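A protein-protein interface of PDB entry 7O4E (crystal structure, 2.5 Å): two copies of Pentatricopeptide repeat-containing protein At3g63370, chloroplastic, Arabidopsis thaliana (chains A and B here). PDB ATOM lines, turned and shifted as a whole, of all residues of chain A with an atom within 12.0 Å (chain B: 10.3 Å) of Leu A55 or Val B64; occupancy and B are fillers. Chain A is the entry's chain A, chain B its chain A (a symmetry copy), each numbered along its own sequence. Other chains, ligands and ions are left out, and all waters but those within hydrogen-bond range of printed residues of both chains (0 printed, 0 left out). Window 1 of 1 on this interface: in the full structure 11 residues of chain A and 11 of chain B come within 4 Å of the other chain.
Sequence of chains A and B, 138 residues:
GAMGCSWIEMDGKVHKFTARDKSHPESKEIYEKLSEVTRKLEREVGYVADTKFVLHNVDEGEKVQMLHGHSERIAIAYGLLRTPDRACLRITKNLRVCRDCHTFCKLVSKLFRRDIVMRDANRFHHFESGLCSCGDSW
N of Glu A60 lies within hydrogen-bond range of SD of Met B66, at 3.3 Å. The backbone carbonyl oxygen (O) of Val B64 sits close to the backbone NH (N) of Gly A61 (3.2 Å). The backbone carbonyl oxygen of Glu A62 lies within hydrogen-bond range of the backbone NH of Val B64 (2.7 Å). O of Val A64 sits close to N of Gly B61, 3.2 Å away. N of Val A64 lies within hydrogen-bond range of O of Glu B62 (2.7 Å). The side-chain sulfur of Met A66 sits at hydrogen-bond distance from the backbone NH of Glu B60, 3.3 Å away.
Among the printed residues, pairs that only touch across the chains: Thr A51 with Val B58 (3.7 Å), Phe A53 with Leu B55 (3.96 Å), Phe A53 with Val B58 (3.5 Å), Leu A55 with Phe B53 (3.96 Å), Leu A55 with Val B64 (3.7 Å), Val A58 with Thr B51 (3.7 Å), Val A58 with Phe B53 (3.5 Å), Val A58 with Val B64 (3.2 Å), Val A58 with Met B66 (3.9 Å), Glu A62 with Glu B62 (3.9 Å), Glu A62 with Lys B63 (3.3 Å), Lys A63 with Glu B62 (3.3 Å), Lys A63 with Lys B63 (3.9 Å), Val A64 with Leu B55 (3.7 Å), Val A64 with Val B58 (3.2 Å) and Met A66 with Val B58 (3.9 Å).
Leu A55 touches just these residues of chain B: Phe B53 and Val B64. Of chain A, only Leu A55, Val A58, Gly A61 and Glu A62 come within 4 Å of Val B64. No residue of chain B comes within 4 Å of Val A54. No residue of chain B comes within 4 Å of His A56. Val A64 touches just these residues of chain B: Leu B55, Val B58, Gly B61 and Glu B62. Phe B53 touches just these residues of chain A: Leu A55 and Val A58. Of the printed residues of chain A, Lys B63 touches Glu A62 and Lys A63. No residue of chain A comes within 4 Å of Gln B65. Of the printed residues of chain A, Glu B60 touches Met A66 (3.3 Å). Printed residues of chain B within 4 Å of Glu A62: Glu B62 (3.9 Å), Lys B63 (3.3 Å) and Val B64 (2.7 Å). Of the printed residues of chain A, Leu B55 touches Phe A53 and Val A64. Asn B57 touches none of the printed residues of chain A. The nearest residue of chain B that does not touch Leu A55 is Leu B55 (5.1 Å). The nearest residue of chain A that does not touch Val B64 is Glu A60 (4.5 Å). The nearest printed residue of chain B that does not touch Phe A53 is Phe B53 (5.5 Å).
Hydrophobic or aromatic side chains of chain B within 4 Å of the printed part of chain A: Phe B53, Leu B55, Val B58, Val B64 and Met B66. Along chain B the printed residues that touch a printed residue of chain A span positions 51 to 66. Among the printed residues, no Asp or Glu carboxylate lies within 4 Å of a Lys or Arg side-chain nitrogen of the other chain.
Phe A53 touches Val B58, and with the chains exchanged Val A58 touches Phe B53. Val A58 touches Val B64, and with the chains exchanged Val A64 touches Val B58. Val A58 touches Met B66, and with the chains exchanged Met A66 touches Val B58. Glu A62 touches Val B64, and with the chains exchanged Val A64 touches Glu B62. Positions printed for both chains: 51, 52, 53, 54, 55, 56, 57, 58, 59, 60, 61, 62, 63, 64, 65, 66, 67 and 68. Of the 22 pairs that touch across the chains among the printed residues, 22 have their exchanged pair printed and touching as well.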
ATOM      1  N   THR A  51      18.037  25.484   2.845  1.00  0.00           N
ATOM      2  CA  THR A  51      18.158  24.305   3.692  1.00  0.00           C
ATOM      3  C   THR A  51      19.537  24.295   4.340  1.00  0.00           C
ATOM      4  O   THR A  51      20.555  24.212   3.643  1.00  0.00           O
ATOM      5  CB  THR A  51      17.933  23.034   2.875  1.00  0.00           C
ATOM      6  OG1 THR A  51      16.706  23.142   2.142  1.00  0.00           O
ATOM      7  CG2 THR A  51      17.863  21.816   3.786  1.00  0.00           C
ATOM      8  N   LYS A  52      19.574  24.400   5.665  1.00  0.00           N
ATOM      9  CA  LYS A  52      20.805  24.292   6.434  1.00  0.00           C
ATOM     10  C   LYS A  52      20.706  23.090   7.362  1.00  0.00           C
ATOM     11  O   LYS A  52      19.654  22.844   7.960  1.00  0.00           O
ATOM     12  CB  LYS A  52      21.082  25.560   7.256  1.00  0.00           C
ATOM     13  CG  LYS A  52      21.382  26.815   6.445  1.00  0.00           C
ATOM     14  CD  LYS A  52      22.151  27.828   7.291  1.00  0.00           C
ATOM     15  CE  LYS A  52      22.216  29.201   6.637  1.00  0.00           C
ATOM     16  NZ  LYS A  52      20.934  29.952   6.762  1.00  0.00           N
ATOM     17  N   PHE A  53      21.804  22.346   7.479  1.00  0.00           N
ATOM     18  CA  PHE A  53      21.831  21.151   8.309  1.00  0.00           C
ATOM     19  C   PHE A  53      23.265  20.879   8.741  1.00  0.00           C
ATOM     20  O   PHE A  53      24.218  21.462   8.219  1.00  0.00           O
ATOM     21  CB  PHE A  53      21.251  19.941   7.570  1.00  0.00           C
ATOM     22  CG  PHE A  53      22.058  19.516   6.372  1.00  0.00           C
ATOM     23  CD1 PHE A  53      21.938  20.186   5.167  1.00  0.00           C
ATOM     24  CD2 PHE A  53      22.932  18.443   6.451  1.00  0.00           C
ATOM     25  CE1 PHE A  53      22.674  19.796   4.063  1.00  0.00           C
ATOM     26  CE2 PHE A  53      23.674  18.050   5.351  1.00  0.00           C
ATOM     27  CZ  PHE A  53      23.542  18.727   4.156  1.00  0.00           C
ATOM     28  N   VAL A  54      23.409  19.974   9.708  1.00  0.00           N
ATOM     29  CA  VAL A  54      24.717  19.535  10.172  1.00  0.00           C
ATOM     30  C   VAL A  54      24.802  18.020  10.067  1.00  0.00           C
ATOM     31  O   VAL A  54      23.796  17.306  10.063  1.00  0.00           O
ATOM     32  CB  VAL A  54      25.025  19.979  11.618  1.00  0.00           C
ATOM     33  CG1 VAL A  54      25.774  21.300  11.625  1.00  0.00           C
ATOM     34  CG2 VAL A  54      23.747  20.072  12.431  1.00  0.00           C
ATOM     35  N   LEU A  55      26.036  17.539   9.971  1.00  0.00           N
ATOM     36  CA  LEU A  55      26.363  16.133  10.156  1.00  0.00           C
ATOM     37  C   LEU A  55      27.499  16.076  11.161  1.00  0.00           C
ATOM     38  O   LEU A  55      28.582  16.611  10.903  1.00  0.00           O
ATOM     39  CB  LEU A  55      26.764  15.464   8.837  1.00  0.00           C
ATOM     40  CG  LEU A  55      25.676  15.360   7.768  1.00  0.00           C
ATOM     41  CD1 LEU A  55      26.266  14.882   6.447  1.00  0.00           C
ATOM     42  CD2 LEU A  55      24.574  14.429   8.234  1.00  0.00           C
ATOM     43  N   HIS A  56      27.243  15.468  12.318  1.00  0.00           N
ATOM     44  CA  HIS A  56      28.285  15.380  13.335  1.00  0.00           C
ATOM     45  C   HIS A  56      29.450  14.520  12.861  1.00  0.00           C
ATOM     46  O   HIS A  56      30.585  14.711  13.312  1.00  0.00           O
ATOM     47  CB  HIS A  56      27.695  14.847  14.639  1.00  0.00           C
ATOM     48  CG  HIS A  56      26.619  15.719  15.211  1.00  0.00           C
ATOM     49  ND1 HIS A  56      26.891  16.824  15.989  1.00  0.00           N
ATOM     50  CD2 HIS A  56      25.270  15.653  15.111  1.00  0.00           C
ATOM     51  CE1 HIS A  56      25.756  17.398  16.347  1.00  0.00           C
ATOM     52  NE2 HIS A  56      24.758  16.706  15.827  1.00  0.00           N
ATOM     53  N   ASN A  57      29.188  13.579  11.956  1.00  0.00           N
ATOM     54  CA  ASN A  57      30.236  12.849  11.250  1.00  0.00           C
ATOM     55  C   ASN A  57      29.661  12.446   9.904  1.00  0.00           C
ATOM     56  O   ASN A  57      28.624  11.782   9.850  1.00  0.00           O
ATOM     57  CB  ASN A  57      30.705  11.620  12.037  1.00  0.00           C
ATOM     58  CG  ASN A  57      31.950  10.980  11.437  1.00  0.00           C
ATOM     59  OD1 ASN A  57      32.551  11.516  10.504  1.00  0.00           O
ATOM     60  ND2 ASN A  57      32.345   9.832  11.977  1.00  0.00           N
ATOM     61  N   VAL A  58      30.315  12.857   8.820  1.00  0.00           N
ATOM     62  CA  VAL A  58      29.761  12.597   7.497  1.00  0.00           C
ATOM     63  C   VAL A  58      29.804  11.108   7.179  1.00  0.00           C
ATOM     64  O   VAL A  58      28.878  10.558   6.573  1.00  0.00           O
ATOM     65  CB  VAL A  58      30.509  13.431   6.441  1.00  0.00           C
ATOM     66  CG1 VAL A  58      30.100  13.013   5.036  1.00  0.00           C
ATOM     67  CG2 VAL A  58      30.232  14.909   6.660  1.00  0.00           C
ATOM     68  N   ASP A  59      30.860  10.426   7.610  1.00  0.00           N
ATOM     69  CA  ASP A  59      31.139   9.080   7.126  1.00  0.00           C
ATOM     70  C   ASP A  59      30.132   8.073   7.656  1.00  0.00           C
ATOM     71  O   ASP A  59      29.936   7.957   8.867  1.00  0.00           O
ATOM     72  CB  ASP A  59      32.543   8.644   7.538  1.00  0.00           C
ATOM     73  CG  ASP A  59      33.608   9.564   7.016  1.00  0.00           C
ATOM     74  OD1 ASP A  59      33.460  10.789   7.219  1.00  0.00           O
ATOM     75  OD2 ASP A  59      34.583   9.066   6.410  1.00  0.00           O
ATOM     76  N   GLU A  60      29.488   7.354   6.735  1.00  0.00           N
ATOM     77  CA  GLU A  60      28.926   6.028   6.982  1.00  0.00           C
ATOM     78  C   GLU A  60      27.717   6.073   7.930  1.00  0.00           C
ATOM     79  O   GLU A  60      27.788   5.687   9.095  1.00  0.00           O
ATOM     80  CB  GLU A  60      30.025   5.101   7.518  1.00  0.00           C
ATOM     81  CG  GLU A  60      31.201   4.908   6.562  1.00  0.00           C
ATOM     82  CD  GLU A  60      32.263   3.997   7.127  1.00  0.00           C
ATOM     83  OE1 GLU A  60      33.293   4.511   7.614  1.00  0.00           O
ATOM     84  OE2 GLU A  60      32.059   2.766   7.086  1.00  0.00           O
ATOM     85  N   GLY A  61      26.597   6.548   7.384  1.00  0.00           N
ATOM     86  CA  GLY A  61      25.295   6.295   7.977  1.00  0.00           C
ATOM     87  C   GLY A  61      24.821   7.232   9.068  1.00  0.00           C
ATOM     88  O   GLY A  61      23.866   6.886   9.780  1.00  0.00           O
ATOM     89  N   GLU A  62      25.433   8.400   9.224  1.00  0.00           N
ATOM     90  CA  GLU A  62      24.972   9.329  10.240  1.00  0.00           C
ATOM     91  C   GLU A  62      23.657   9.968   9.808  1.00  0.00           C
ATOM     92  O   GLU A  62      23.318  10.019   8.623  1.00  0.00           O
ATOM     93  CB  GLU A  62      26.025  10.403  10.494  1.00  0.00           C
ATOM     94  CG  GLU A  62      25.982  11.012  11.884  1.00  0.00           C
ATOM     95  CD  GLU A  62      26.826  10.247  12.889  1.00  0.00           C
ATOM     96  OE1 GLU A  62      27.825   9.622  12.474  1.00  0.00           O
ATOM     97  OE2 GLU A  62      26.495  10.276  14.094  1.00  0.00           O
ATOM     98  N   LYS A  63      22.906  10.452  10.790  1.00  0.00           N
ATOM     99  CA  LYS A  63      21.633  11.100  10.530  1.00  0.00           C
ATOM    100  C   LYS A  63      21.827  12.595  10.291  1.00  0.00           C
ATOM    101  O   LYS A  63      22.818  13.198  10.713  1.00  0.00           O
ATOM    102  CB  LYS A  63      20.667  10.876  11.692  1.00  0.00           C
ATOM    103  CG  LYS A  63      19.973   9.522  11.676  1.00  0.00           C
ATOM    104  CD  LYS A  63      18.965   9.405  12.810  1.00  0.00           C
ATOM    105  CE  LYS A  63      18.138   8.134  12.688  1.00  0.00           C
ATOM    106  NZ  LYS A  63      17.115   8.033  13.766  1.00  0.00           N
ATOM    107  N   VAL A  64      20.858  13.189   9.602  1.00  0.00           N
ATOM    108  CA  VAL A  64      20.882  14.613   9.297  1.00  0.00           C
ATOM    109  C   VAL A  64      20.189  15.373  10.418  1.00  0.00           C
ATOM    110  O   VAL A  64      19.081  15.019  10.834  1.00  0.00           O
ATOM    111  CB  VAL A  64      20.213  14.900   7.943  1.00  0.00           C
ATOM    112  CG1 VAL A  64      19.901  16.386   7.813  1.00  0.00           C
ATOM    113  CG2 VAL A  64      21.113  14.451   6.810  1.00  0.00           C
ATOM    114  N   GLN A  65      20.844  16.420  10.906  1.00  0.00           N
ATOM    115  CA  GLN A  65      20.293  17.292  11.934  1.00  0.00           C
ATOM    116  C   GLN A  65      20.135  18.683  11.336  1.00  0.00           C
ATOM    117  O   GLN A  65      21.111  19.268  10.855  1.00  0.00           O
ATOM    118  CB  GLN A  65      21.204  17.315  13.164  1.00  0.00           C
ATOM    119  CG  GLN A  65      20.727  18.197  14.304  1.00  0.00           C
ATOM    120  CD  GLN A  65      21.608  18.068  15.534  1.00  0.00           C
ATOM    121  OE1 GLN A  65      22.025  16.967  15.898  1.00  0.00           O
ATOM    122  NE2 GLN A  65      21.904  19.195  16.174  1.00  0.00           N
ATOM    123  N   MET A  66      18.910  19.200  11.343  1.00  0.00           N
ATOM    124  CA  MET A  66      18.649  20.517  10.780  1.00  0.00           C
ATOM    125  C   MET A  66      19.093  21.617  11.741  1.00  0.00           C
ATOM    126  O   MET A  66      19.022  21.473  12.965  1.00  0.00           O
ATOM    127  CB  MET A  66      17.165  20.675  10.449  1.00  0.00           C
ATOM    128  CG  MET A  66      16.626  19.577   9.544  1.00  0.00           C
ATOM    129  SD  MET A  66      17.488  19.479   7.959  1.00  0.00           S
ATOM    130  CE  MET A  66      16.899  20.961   7.148  1.00  0.00           C
ATOM    131  N   LEU A  67      19.559  22.727  11.167  1.00  0.00           N
ATOM    132  CA  LEU A  67      20.086  23.824  11.972  1.00  0.00           C
ATOM    133  C   LEU A  67      18.986  24.718  12.525  1.00  0.00           C
ATOM    134  O   LEU A  67      19.160  25.320  13.590  1.00  0.00           O
ATOM    135  CB  LEU A  67      21.069  24.653  11.143  1.00  0.00           C
ATOM    136  CG  LEU A  67      22.541  24.644  11.571  1.00  0.00           C
ATOM    137  CD1 LEU A  67      22.811  23.596  12.647  1.00  0.00           C
ATOM    138  CD2 LEU A  67      23.452  24.425  10.367  1.00  0.00           C
ATOM    139  N   HIS A  68      17.858  24.821  11.827  1.00  0.00           N
ATOM    140  CA  HIS A  68      16.742  25.652  12.261  1.00  0.00           C
ATOM    141  C   HIS A  68      15.472  24.818  12.233  1.00  0.00           C
ATOM    142  O   HIS A  68      15.119  24.255  11.191  1.00  0.00           O
ATOM    143  CB  HIS A  68      16.595  26.888  11.373  1.00  0.00           C
ATOM    144  CG  HIS A  68      17.769  27.812  11.430  1.00  0.00           C
ATOM    145  ND1 HIS A  68      18.137  28.476  12.581  1.00  0.00           N
ATOM    146  CD2 HIS A  68      18.656  28.188  10.480  1.00  0.00           C
ATOM    147  CE1 HIS A  68      19.201  29.219  12.337  1.00  0.00           C
ATOM    148  NE2 HIS A  68      19.536  29.063  11.069  1.00  0.00           N
ATOM    149  N   THR B  51      35.571  12.385   0.532  1.00  0.00           N
ATOM    150  CA  THR B  51      34.336  11.829   1.069  1.00  0.00           C
ATOM    151  C   THR B  51      33.182  12.190   0.142  1.00  0.00           C
ATOM    152  O   THR B  51      32.870  13.373  -0.039  1.00  0.00           O
ATOM    153  CB  THR B  51      34.082  12.354   2.481  1.00  0.00           C
ATOM    154  OG1 THR B  51      35.250  12.154   3.288  1.00  0.00           O
ATOM    155  CG2 THR B  51      32.905  11.629   3.119  1.00  0.00           C
ATOM    156  N   LYS B  52      32.564  11.178  -0.461  1.00  0.00           N
ATOM    157  CA  LYS B  52      31.376  11.354  -1.284  1.00  0.00           C
ATOM    158  C   LYS B  52      30.218  10.597  -0.650  1.00  0.00           C
ATOM    159  O   LYS B  52      30.393   9.478  -0.159  1.00  0.00           O
ATOM    160  CB  LYS B  52      31.594  10.858  -2.721  1.00  0.00           C
ATOM    161  CG  LYS B  52      32.607  11.648  -3.541  1.00  0.00           C
ATOM    162  CD  LYS B  52      32.360  11.448  -5.035  1.00  0.00           C
ATOM    163  CE  LYS B  52      33.509  11.966  -5.889  1.00  0.00           C
ATOM    164  NZ  LYS B  52      34.683  11.048  -5.880  1.00  0.00           N
ATOM    165  N   PHE B  53      29.036  11.211  -0.664  1.00  0.00           N
ATOM    166  CA  PHE B  53      27.856  10.610  -0.062  1.00  0.00           C
ATOM    167  C   PHE B  53      26.613  11.179  -0.730  1.00  0.00           C
ATOM    168  O   PHE B  53      26.670  12.169  -1.462  1.00  0.00           O
ATOM    169  CB  PHE B  53      27.814  10.850   1.451  1.00  0.00           C
ATOM    170  CG  PHE B  53      27.663  12.298   1.833  1.00  0.00           C
ATOM    171  CD1 PHE B  53      28.757  13.146   1.828  1.00  0.00           C
ATOM    172  CD2 PHE B  53      26.429  12.810   2.201  1.00  0.00           C
ATOM    173  CE1 PHE B  53      28.625  14.476   2.182  1.00  0.00           C
ATOM    174  CE2 PHE B  53      26.289  14.141   2.553  1.00  0.00           C
ATOM    175  CZ  PHE B  53      27.390  14.974   2.545  1.00  0.00           C
ATOM    176  N   VAL B  54      25.476  10.537  -0.464  1.00  0.00           N
ATOM    177  CA  VAL B  54      24.187  11.006  -0.951  1.00  0.00           C
ATOM    178  C   VAL B  54      23.239  11.176   0.225  1.00  0.00           C
ATOM    179  O   VAL B  54      23.394  10.566   1.286  1.00  0.00           O
ATOM    180  CB  VAL B  54      23.558  10.063  -2.000  1.00  0.00           C
ATOM    181  CG1 VAL B  54      23.936  10.496  -3.406  1.00  0.00           C
ATOM    182  CG2 VAL B  54      23.974   8.627  -1.742  1.00  0.00           C
ATOM    183  N   LEU B  55      22.248  12.037   0.020  1.00  0.00           N
ATOM    184  CA  LEU B  55      21.079  12.130   0.881  1.00  0.00           C
ATOM    185  C   LEU B  55      19.862  12.061  -0.024  1.00  0.00           C
ATOM    186  O   LEU B  55      19.679  12.928  -0.884  1.00  0.00           O
ATOM    187  CB  LEU B  55      21.079  13.424   1.701  1.00  0.00           C
ATOM    188  CG  LEU B  55      22.198  13.577   2.731  1.00  0.00           C
ATOM    189  CD1 LEU B  55      22.207  14.986   3.309  1.00  0.00           C
ATOM    190  CD2 LEU B  55      22.040  12.545   3.830  1.00  0.00           C
ATOM    191  N   HIS B  56      19.055  11.013   0.139  1.00  0.00           N
ATOM    192  CA  HIS B  56      17.869  10.877  -0.699  1.00  0.00           C
ATOM    193  C   HIS B  56      16.870  11.996  -0.432  1.00  0.00           C
ATOM    194  O   HIS B  56      16.086  12.352  -1.318  1.00  0.00           O
ATOM    195  CB  HIS B  56      17.236   9.503  -0.484  1.00  0.00           C
ATOM    196  CG  HIS B  56      18.139   8.364  -0.841  1.00  0.00           C
ATOM    197  ND1 HIS B  56      18.281   7.903  -2.133  1.00  0.00           N
ATOM    198  CD2 HIS B  56      18.954   7.598  -0.078  1.00  0.00           C
ATOM    199  CE1 HIS B  56      19.140   6.899  -2.148  1.00  0.00           C
ATOM    200  NE2 HIS B  56      19.563   6.694  -0.914  1.00  0.00           N
ATOM    201  N   ASN B  57      16.890  12.559   0.775  1.00  0.00           N
ATOM    202  CA  ASN B  57      16.158  13.782   1.087  1.00  0.00           C
ATOM    203  C   ASN B  57      16.922  14.480   2.199  1.00  0.00           C
ATOM    204  O   ASN B  57      17.152  13.887   3.255  1.00  0.00           O
ATOM    205  CB  ASN B  57      14.714  13.493   1.512  1.00  0.00           C
ATOM    206  CG  ASN B  57      13.869  14.755   1.616  1.00  0.00           C
ATOM    207  OD1 ASN B  57      14.312  15.846   1.252  1.00  0.00           O
ATOM    208  ND2 ASN B  57      12.643  14.608   2.107  1.00  0.00           N
ATOM    209  N   VAL B  58      17.331  15.724   1.963  1.00  0.00           N
ATOM    210  CA  VAL B  58      18.161  16.413   2.944  1.00  0.00           C
ATOM    211  C   VAL B  58      17.360  16.723   4.202  1.00  0.00           C
ATOM    212  O   VAL B  58      17.871  16.626   5.324  1.00  0.00           O
ATOM    213  CB  VAL B  58      18.764  17.685   2.321  1.00  0.00           C
ATOM    214  CG1 VAL B  58      19.448  18.532   3.384  1.00  0.00           C
ATOM    215  CG2 VAL B  58      19.746  17.307   1.226  1.00  0.00           C
ATOM    216  N   ASP B  59      16.086  17.065   4.042  1.00  0.00           N
ATOM    217  CA  ASP B  59      15.318  17.648   5.134  1.00  0.00           C
ATOM    218  C   ASP B  59      15.023  16.627   6.221  1.00  0.00           C
ATOM    219  O   ASP B  59      14.462  15.564   5.950  1.00  0.00           O
ATOM    220  CB  ASP B  59      13.999  18.217   4.616  1.00  0.00           C
ATOM    221  CG  ASP B  59      14.200  19.270   3.565  1.00  0.00           C
ATOM    222  OD1 ASP B  59      14.955  18.991   2.609  1.00  0.00           O
ATOM    223  OD2 ASP B  59      13.608  20.365   3.695  1.00  0.00           O
ATOM    224  N   GLU B  60      15.418  16.957   7.452  1.00  0.00           N
ATOM    225  CA  GLU B  60      14.798  16.443   8.672  1.00  0.00           C
ATOM    226  C   GLU B  60      15.075  14.946   8.883  1.00  0.00           C
ATOM    227  O   GLU B  60      14.208  14.092   8.705  1.00  0.00           O
ATOM    228  CB  GLU B  60      13.293  16.737   8.641  1.00  0.00           C
ATOM    229  CG  GLU B  60      12.946  18.223   8.566  1.00  0.00           C
ATOM    230  CD  GLU B  60      11.458  18.470   8.531  1.00  0.00           C
ATOM    231  OE1 GLU B  60      10.922  18.724   7.431  1.00  0.00           O
ATOM    232  OE2 GLU B  60      10.828  18.402   9.607  1.00  0.00           O
ATOM    233  N   GLY B  61      16.315  14.658   9.279  1.00  0.00           N
ATOM    234  CA  GLY B  61      16.639  13.386   9.902  1.00  0.00           C
ATOM    235  C   GLY B  61      16.963  12.217   8.995  1.00  0.00           C
ATOM    236  O   GLY B  61      16.962  11.073   9.472  1.00  0.00           O
ATOM    237  N   GLU B  62      17.252  12.452   7.721  1.00  0.00           N
ATOM    238  CA  GLU B  62      17.602  11.351   6.842  1.00  0.00           C
ATOM    239  C   GLU B  62      19.005  10.848   7.166  1.00  0.00           C
ATOM    240  O   GLU B  62      19.832  11.557   7.745  1.00  0.00           O
ATOM    241  CB  GLU B  62      17.519  11.788   5.383  1.00  0.00           C
ATOM    242  CG  GLU B  62      17.232  10.665   4.404  1.00  0.00           C
ATOM    243  CD  GLU B  62      15.746  10.429   4.197  1.00  0.00           C
ATOM    244  OE1 GLU B  62      14.964  11.393   4.341  1.00  0.00           O
ATOM    245  OE2 GLU B  62      15.359   9.282   3.882  1.00  0.00           O
ATOM    246  N   LYS B  63      19.266   9.601   6.793  1.00  0.00           N
ATOM    247  CA  LYS B  63      20.563   8.990   7.022  1.00  0.00           C
ATOM    248  C   LYS B  63      21.504   9.263   5.851  1.00  0.00           C
ATOM    249  O   LYS B  63      21.078   9.542   4.727  1.00  0.00           O
ATOM    250  CB  LYS B  63      20.418   7.485   7.239  1.00  0.00           C
ATOM    251  CG  LYS B  63      19.993   7.094   8.647  1.00  0.00           C
ATOM    252  CD  LYS B  63      19.955   5.582   8.811  1.00  0.00           C
ATOM    253  CE  LYS B  63      19.713   5.188  10.261  1.00  0.00           C
ATOM    254  NZ  LYS B  63      19.723   3.709  10.442  1.00  0.00           N
ATOM    255  N   VAL B  64      22.799   9.178   6.135  1.00  0.00           N
ATOM    256  CA  VAL B  64      23.830   9.398   5.129  1.00  0.00           C
ATOM    257  C   VAL B  64      24.161   8.073   4.459  1.00  0.00           C
ATOM    258  O   VAL B  64      24.393   7.063   5.131  1.00  0.00           O
ATOM    259  CB  VAL B  64      25.088  10.026   5.754  1.00  0.00           C
ATOM    260  CG1 VAL B  64      26.270   9.897   4.802  1.00  0.00           C
ATOM    261  CG2 VAL B  64      24.834  11.483   6.084  1.00  0.00           C
ATOM    262  N   GLN B  65      24.181   8.079   3.131  1.00  0.00           N
ATOM    263  CA  GLN B  65      24.544   6.913   2.338  1.00  0.00           C
ATOM    264  C   GLN B  65      25.809   7.247   1.561  1.00  0.00           C
ATOM    265  O   GLN B  65      25.833   8.219   0.800  1.00  0.00           O
ATOM    266  CB  GLN B  65      23.399   6.525   1.398  1.00  0.00           C
ATOM    267  CG  GLN B  65      23.667   5.318   0.518  1.00  0.00           C
ATOM    268  CD  GLN B  65      22.445   4.916  -0.288  1.00  0.00           C
ATOM    269  OE1 GLN B  65      21.324   4.919   0.222  1.00  0.00           O
ATOM    270  NE2 GLN B  65      22.655   4.577  -1.557  1.00  0.00           N
ATOM    271  N   MET B  66      26.862   6.461   1.767  1.00  0.00           N
ATOM    272  CA  MET B  66      28.125   6.706   1.086  1.00  0.00           C
ATOM    273  C   MET B  66      28.069   6.210  -0.357  1.00  0.00           C
ATOM    274  O   MET B  66      27.409   5.216  -0.674  1.00  0.00           O
ATOM    275  CB  MET B  66      29.276   6.030   1.831  1.00  0.00           C
ATOM    276  CG  MET B  66      29.363   6.423   3.297  1.00  0.00           C
ATOM    277  SD  MET B  66      29.578   8.199   3.544  1.00  0.00           S
ATOM    278  CE  MET B  66      31.265   8.427   2.992  1.00  0.00           C
ATOM    279  N   LEU B  67      28.774   6.923  -1.237  1.00  0.00           N
ATOM    280  CA  LEU B  67      28.743   6.601  -2.660  1.00  0.00           C
ATOM    281  C   LEU B  67      29.685   5.460  -3.015  1.00  0.00           C
ATOM    282  O   LEU B  67      29.427   4.726  -3.975  1.00  0.00           O
ATOM    283  CB  LEU B  67      29.091   7.844  -3.482  1.00  0.00           C
ATOM    284  CG  LEU B  67      27.991   8.434  -4.373  1.00  0.00           C
ATOM    285  CD1 LEU B  67      26.635   7.789  -4.100  1.00  0.00           C
ATOM    286  CD2 LEU B  67      27.911   9.947  -4.201  1.00  0.00           C
ATOM    287  N   HIS B  68      30.773   5.295  -2.268  1.00  0.00           N
ATOM    288  CA  HIS B  68      31.744   4.238  -2.521  1.00  0.00           C
ATOM    289  C   HIS B  68      31.994   3.483  -1.226  1.00  0.00           C
ATOM    290  O   HIS B  68      32.373   4.086  -0.217  1.00  0.00           O
ATOM    291  CB  HIS B  68      33.050   4.808  -3.073  1.00  0.00           C
ATOM    292  CG  HIS B  68      32.899   5.478  -4.402  1.00  0.00           C
ATOM    293  ND1 HIS B  68      32.520   4.797  -5.539  1.00  0.00           N
ATOM    294  CD2 HIS B  68      33.081   6.765  -4.778  1.00  0.00           C
ATOM    295  CE1 HIS B  68      32.472   5.637  -6.557  1.00  0.00           C
ATOM    296  NE2 HIS B  68      32.808   6.838  -6.122  1.00  0.00           N
